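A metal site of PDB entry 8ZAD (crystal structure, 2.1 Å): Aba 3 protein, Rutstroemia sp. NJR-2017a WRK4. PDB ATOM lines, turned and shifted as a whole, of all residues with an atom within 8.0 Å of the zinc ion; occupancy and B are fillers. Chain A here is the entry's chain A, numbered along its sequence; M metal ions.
The side-chain sulfur (SG) of Cys 372 lies close to the backbone NH (N) of Glu 374.
SG of Cys 349 sits close to N of Lys 351 (3.4 Å).
The side-chain hydroxyl (OH) of Tyr 354 lies within hydrogen-bond range of the backbone NH (N) of Cys 349 (3.0 Å).
Within 4 Å of the zinc ion: Cys 349, Cys 352, Cys 372 and Cys 375.
The nearest printed residue that does not touch the zinc ion is Lys 351 (4.3 Å).
The zinc ion is bound by SG of Cys 349, 2.3 Å away.
SG of Cys 352 is bound to the zinc ion (2.3 Å).
The zinc ion is bound by SG of Cys 372, 2.3 Å away.
The side-chain sulfur (SG) of Cys 375 binds the zinc ion (2.4 Å).
The zinc ion has four donor atoms within binding distance.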
ATOM      1  N   ALA A 157     -10.942 -14.072 -16.764  1.00  0.00           N
ATOM      2  CA  ALA A 157     -11.263 -13.155 -17.888  1.00  0.00           C
ATOM      3  C   ALA A 157     -10.336 -11.926 -17.863  1.00  0.00           C
ATOM      4  O   ALA A 157     -10.559 -11.005 -18.676  1.00  0.00           O
ATOM      5  CB  ALA A 157     -12.714 -12.761 -17.814  1.00  0.00           C
ATOM      6  N   GLN A 158      -9.327 -11.859 -16.986  1.00  0.00           N
ATOM      7  CA  GLN A 158      -8.512 -10.629 -16.866  1.00  0.00           C
ATOM      8  C   GLN A 158      -7.546 -10.491 -18.059  1.00  0.00           C
ATOM      9  O   GLN A 158      -7.197  -9.357 -18.406  1.00  0.00           O
ATOM     10  CB  GLN A 158      -7.807 -10.541 -15.527  1.00  0.00           C
ATOM     11  CG  GLN A 158      -6.677 -11.514 -15.347  1.00  0.00           C
ATOM     12  CD  GLN A 158      -6.239 -11.460 -13.913  1.00  0.00           C
ATOM     13  OE1 GLN A 158      -5.607 -10.490 -13.499  1.00  0.00           O
ATOM     14  NE2 GLN A 158      -6.609 -12.493 -13.162  1.00  0.00           N
ATOM     15  N   VAL A 348     -11.138  -6.649 -13.627  1.00  0.00           N
ATOM     16  CA  VAL A 348     -10.224  -5.507 -13.945  1.00  0.00           C
ATOM     17  C   VAL A 348     -10.878  -4.519 -14.940  1.00  0.00           C
ATOM     18  O   VAL A 348     -10.463  -3.367 -14.943  1.00  0.00           O
ATOM     19  CB  VAL A 348      -8.896  -6.019 -14.537  1.00  0.00           C
ATOM     20  CG1 VAL A 348      -8.189  -7.013 -13.613  1.00  0.00           C
ATOM     21  CG2 VAL A 348      -9.111  -6.642 -15.903  1.00  0.00           C
ATOM     22  N   CYS A 349     -11.776  -4.955 -15.807  1.00  0.00           N
ATOM     23  CA  CYS A 349     -12.337  -4.107 -16.905  1.00  0.00           C
ATOM     24  C   CYS A 349     -13.752  -3.635 -16.523  1.00  0.00           C
ATOM     25  O   CYS A 349     -14.573  -4.494 -16.201  1.00  0.00           O
ATOM     26  CB  CYS A 349     -12.404  -4.877 -18.215  1.00  0.00           C
ATOM     27  SG  CYS A 349     -13.106  -3.938 -19.595  1.00  0.00           S
ATOM     28  N   ASP A 350     -14.013  -2.329 -16.602  1.00  0.00           N
ATOM     29  CA  ASP A 350     -15.322  -1.710 -16.242  1.00  0.00           C
ATOM     30  C   ASP A 350     -16.389  -1.953 -17.311  1.00  0.00           C
ATOM     31  O   ASP A 350     -17.541  -1.560 -17.092  1.00  0.00           O
ATOM     32  CB  ASP A 350     -15.158  -0.199 -16.054  1.00  0.00           C
ATOM     33  CG  ASP A 350     -14.522   0.156 -14.730  1.00  0.00           C
ATOM     34  OD1 ASP A 350     -14.550  -0.706 -13.822  1.00  0.00           O
ATOM     35  OD2 ASP A 350     -14.006   1.289 -14.608  1.00  0.00           O
ATOM     36  N   LYS A 351     -16.016  -2.516 -18.464  1.00  0.00           N
ATOM     37  CA  LYS A 351     -16.953  -2.683 -19.596  1.00  0.00           C
ATOM     38  C   LYS A 351     -17.386  -4.150 -19.717  1.00  0.00           C
ATOM     39  O   LYS A 351     -18.464  -4.380 -20.250  1.00  0.00           O
ATOM     40  CB  LYS A 351     -16.285  -2.128 -20.861  1.00  0.00           C
ATOM     41  CG  LYS A 351     -15.988  -0.634 -20.750  1.00  0.00           C
ATOM     42  CD  LYS A 351     -15.313  -0.083 -21.981  1.00  0.00           C
ATOM     43  CE  LYS A 351     -14.692   1.275 -21.726  1.00  0.00           C
ATOM     44  NZ  LYS A 351     -13.805   1.676 -22.837  1.00  0.00           N
ATOM     45  N   CYS A 352     -16.563  -5.101 -19.275  1.00  0.00           N
ATOM     46  CA  CYS A 352     -16.927  -6.536 -19.284  1.00  0.00           C
ATOM     47  C   CYS A 352     -18.125  -6.761 -18.364  1.00  0.00           C
ATOM     48  O   CYS A 352     -18.344  -5.940 -17.469  1.00  0.00           O
ATOM     49  CB  CYS A 352     -15.757  -7.419 -18.874  1.00  0.00           C
ATOM     50  SG  CYS A 352     -14.474  -7.536 -20.150  1.00  0.00           S
ATOM     51  N   ARG A 353     -18.875  -7.842 -18.567  1.00  0.00           N
ATOM     52  CA  ARG A 353     -20.050  -8.169 -17.715  1.00  0.00           C
ATOM     53  C   ARG A 353     -19.642  -9.260 -16.712  1.00  0.00           C
ATOM     54  O   ARG A 353     -19.476 -10.427 -17.128  1.00  0.00           O
ATOM     55  CB  ARG A 353     -21.247  -8.579 -18.570  1.00  0.00           C
ATOM     56  CG  ARG A 353     -22.534  -8.836 -17.794  1.00  0.00           C
ATOM     57  CD  ARG A 353     -23.585  -9.300 -18.791  1.00  0.00           C
ATOM     58  NE  ARG A 353     -24.846  -9.721 -18.178  1.00  0.00           N
ATOM     59  CZ  ARG A 353     -25.890 -10.195 -18.858  1.00  0.00           C
ATOM     60  NH1 ARG A 353     -26.991 -10.561 -18.208  1.00  0.00           N
ATOM     61  NH2 ARG A 353     -25.845 -10.315 -20.175  1.00  0.00           N
ATOM     62  N   TYR A 354     -19.480  -8.875 -15.451  1.00  0.00           N
ATOM     63  CA  TYR A 354     -19.295  -9.796 -14.316  1.00  0.00           C
ATOM     64  C   TYR A 354     -20.680 -10.119 -13.750  1.00  0.00           C
ATOM     65  O   TYR A 354     -21.697  -9.538 -14.183  1.00  0.00           O
ATOM     66  CB  TYR A 354     -18.260  -9.210 -13.351  1.00  0.00           C
ATOM     67  CG  TYR A 354     -17.008  -8.708 -14.027  1.00  0.00           C
ATOM     68  CD1 TYR A 354     -15.961  -9.570 -14.295  1.00  0.00           C
ATOM     69  CD2 TYR A 354     -16.854  -7.385 -14.417  1.00  0.00           C
ATOM     70  CE1 TYR A 354     -14.810  -9.141 -14.944  1.00  0.00           C
ATOM     71  CE2 TYR A 354     -15.689  -6.939 -15.056  1.00  0.00           C
ATOM     72  CZ  TYR A 354     -14.669  -7.820 -15.331  1.00  0.00           C
ATOM     73  OH  TYR A 354     -13.489  -7.457 -15.951  1.00  0.00           O
ATOM     74  N   VAL A 369     -17.624 -14.755 -17.256  1.00  0.00           N
ATOM     75  CA  VAL A 369     -17.555 -13.328 -17.671  1.00  0.00           C
ATOM     76  C   VAL A 369     -17.866 -13.228 -19.167  1.00  0.00           C
ATOM     77  O   VAL A 369     -17.402 -14.067 -19.942  1.00  0.00           O
ATOM     78  CB  VAL A 369     -16.171 -12.758 -17.345  1.00  0.00           C
ATOM     79  CG1 VAL A 369     -15.974 -11.369 -17.951  1.00  0.00           C
ATOM     80  CG2 VAL A 369     -15.924 -12.746 -15.838  1.00  0.00           C
ATOM     81  N   GLU A 370     -18.619 -12.199 -19.533  1.00  0.00           N
ATOM     82  CA  GLU A 370     -18.872 -11.809 -20.937  1.00  0.00           C
ATOM     83  C   GLU A 370     -17.932 -10.663 -21.307  1.00  0.00           C
ATOM     84  O   GLU A 370     -18.075  -9.559 -20.712  1.00  0.00           O
ATOM     85  CB  GLU A 370     -20.334 -11.387 -21.048  1.00  0.00           C
ATOM     86  CG  GLU A 370     -20.897 -11.512 -22.426  1.00  0.00           C
ATOM     87  CD  GLU A 370     -22.371 -11.200 -22.378  1.00  0.00           C
ATOM     88  OE1 GLU A 370     -23.069 -11.696 -21.439  1.00  0.00           O
ATOM     89  OE2 GLU A 370     -22.809 -10.425 -23.242  1.00  0.00           O
ATOM     90  N   LEU A 371     -16.992 -10.912 -22.203  1.00  0.00           N
ATOM     91  CA  LEU A 371     -15.994  -9.890 -22.584  1.00  0.00           C
ATOM     92  C   LEU A 371     -16.693  -8.760 -23.343  1.00  0.00           C
ATOM     93  O   LEU A 371     -17.554  -9.036 -24.169  1.00  0.00           O
ATOM     94  CB  LEU A 371     -14.900 -10.526 -23.451  1.00  0.00           C
ATOM     95  CG  LEU A 371     -14.043 -11.576 -22.759  1.00  0.00           C
ATOM     96  CD1 LEU A 371     -13.058 -12.136 -23.757  1.00  0.00           C
ATOM     97  CD2 LEU A 371     -13.332 -11.007 -21.533  1.00  0.00           C
ATOM     98  N   CYS A 372     -16.262  -7.523 -23.094  1.00  0.00           N
ATOM     99  CA  CYS A 372     -16.659  -6.321 -23.858  1.00  0.00           C
ATOM    100  C   CYS A 372     -15.953  -6.342 -25.223  1.00  0.00           C
ATOM    101  O   CYS A 372     -15.046  -7.191 -25.424  1.00  0.00           O
ATOM    102  CB  CYS A 372     -16.289  -5.080 -23.075  1.00  0.00           C
ATOM    103  SG  CYS A 372     -14.502  -4.803 -23.007  1.00  0.00           S
ATOM    104  N   SER A 373     -16.349  -5.447 -26.121  1.00  0.00           N
ATOM    105  CA  SER A 373     -15.763  -5.265 -27.472  1.00  0.00           C
ATOM    106  C   SER A 373     -14.238  -5.200 -27.439  1.00  0.00           C
ATOM    107  O   SER A 373     -13.606  -5.887 -28.213  1.00  0.00           O
ATOM    108  CB  SER A 373     -16.302  -4.003 -28.100  1.00  0.00           C
ATOM    109  OG  SER A 373     -17.684  -4.205 -28.241  1.00  0.00           O
ATOM    110  N   GLU A 374     -13.700  -4.290 -26.631  1.00  0.00           N
ATOM    111  CA  GLU A 374     -12.250  -4.025 -26.582  1.00  0.00           C
ATOM    112  C   GLU A 374     -11.497  -5.261 -26.068  1.00  0.00           C
ATOM    113  O   GLU A 374     -10.448  -5.579 -26.643  1.00  0.00           O
ATOM    114  CB  GLU A 374     -11.942  -2.857 -25.650  1.00  0.00           C
ATOM    115  CG  GLU A 374     -12.413  -1.525 -26.179  1.00  0.00           C
ATOM    116  CD  GLU A 374     -12.343  -0.488 -25.072  1.00  0.00           C
ATOM    117  OE1 GLU A 374     -13.406  -0.210 -24.479  1.00  0.00           O
ATOM    118  OE2 GLU A 374     -11.197  -0.072 -24.726  1.00  0.00           O
ATOM    119  N   CYS A 375     -12.047  -5.965 -25.078  1.00  0.00           N
ATOM    120  CA  CYS A 375     -11.399  -7.196 -24.536  1.00  0.00           C
ATOM    121  C   CYS A 375     -11.473  -8.277 -25.623  1.00  0.00           C
ATOM    122  O   CYS A 375     -10.458  -8.872 -25.907  1.00  0.00           O
ATOM    123  CB  CYS A 375     -12.001  -7.602 -23.201  1.00  0.00           C
ATOM    124  SG  CYS A 375     -11.483  -6.530 -21.830  1.00  0.00           S
ATOM    125  N   LYS A 376     -12.598  -8.442 -26.306  1.00  0.00           N
ATOM    126  CA  LYS A 376     -12.692  -9.438 -27.398  1.00  0.00           C
ATOM    127  C   LYS A 376     -11.534  -9.235 -28.383  1.00  0.00           C
ATOM    128  O   LYS A 376     -10.901 -10.252 -28.760  1.00  0.00           O
ATOM    129  CB  LYS A 376     -14.069  -9.343 -28.035  1.00  0.00           C
ATOM    130  CG  LYS A 376     -15.168  -9.986 -27.203  1.00  0.00           C
ATOM    131  CD  LYS A 376     -16.540  -9.870 -27.803  1.00  0.00           C
ATOM    132  CE  LYS A 376     -17.424 -10.986 -27.318  1.00  0.00           C
ATOM    133  NZ  LYS A 376     -18.851 -10.648 -27.455  1.00  0.00           N
ATOM    134  N   TRP A 379      -8.134 -10.286 -26.978  1.00  0.00           N
ATOM    135  CA  TRP A 379      -8.126 -11.762 -26.938  1.00  0.00           C
ATOM    136  C   TRP A 379      -7.992 -12.271 -28.374  1.00  0.00           C
ATOM    137  O   TRP A 379      -7.221 -13.171 -28.557  1.00  0.00           O
ATOM    138  CB  TRP A 379      -9.365 -12.323 -26.241  1.00  0.00           C
ATOM    139  CG  TRP A 379      -9.398 -12.116 -24.764  1.00  0.00           C
ATOM    140  CD1 TRP A 379      -9.390 -10.923 -24.080  1.00  0.00           C
ATOM    141  CD2 TRP A 379      -9.546 -13.150 -23.776  1.00  0.00           C
ATOM    142  NE1 TRP A 379      -9.463 -11.153 -22.741  1.00  0.00           N
ATOM    143  CE2 TRP A 379      -9.576 -12.501 -22.522  1.00  0.00           C
ATOM    144  CE3 TRP A 379      -9.582 -14.539 -23.820  1.00  0.00           C
ATOM    145  CZ2 TRP A 379      -9.719 -13.222 -21.329  1.00  0.00           C
ATOM    146  CZ3 TRP A 379      -9.693 -15.259 -22.646  1.00  0.00           C
ATOM    147  CH2 TRP A 379      -9.787 -14.597 -21.419  1.00  0.00           C
HETATM  148 ZN    ZN M   1     -13.532  -5.639 -21.052  1.00  0.00          ZN
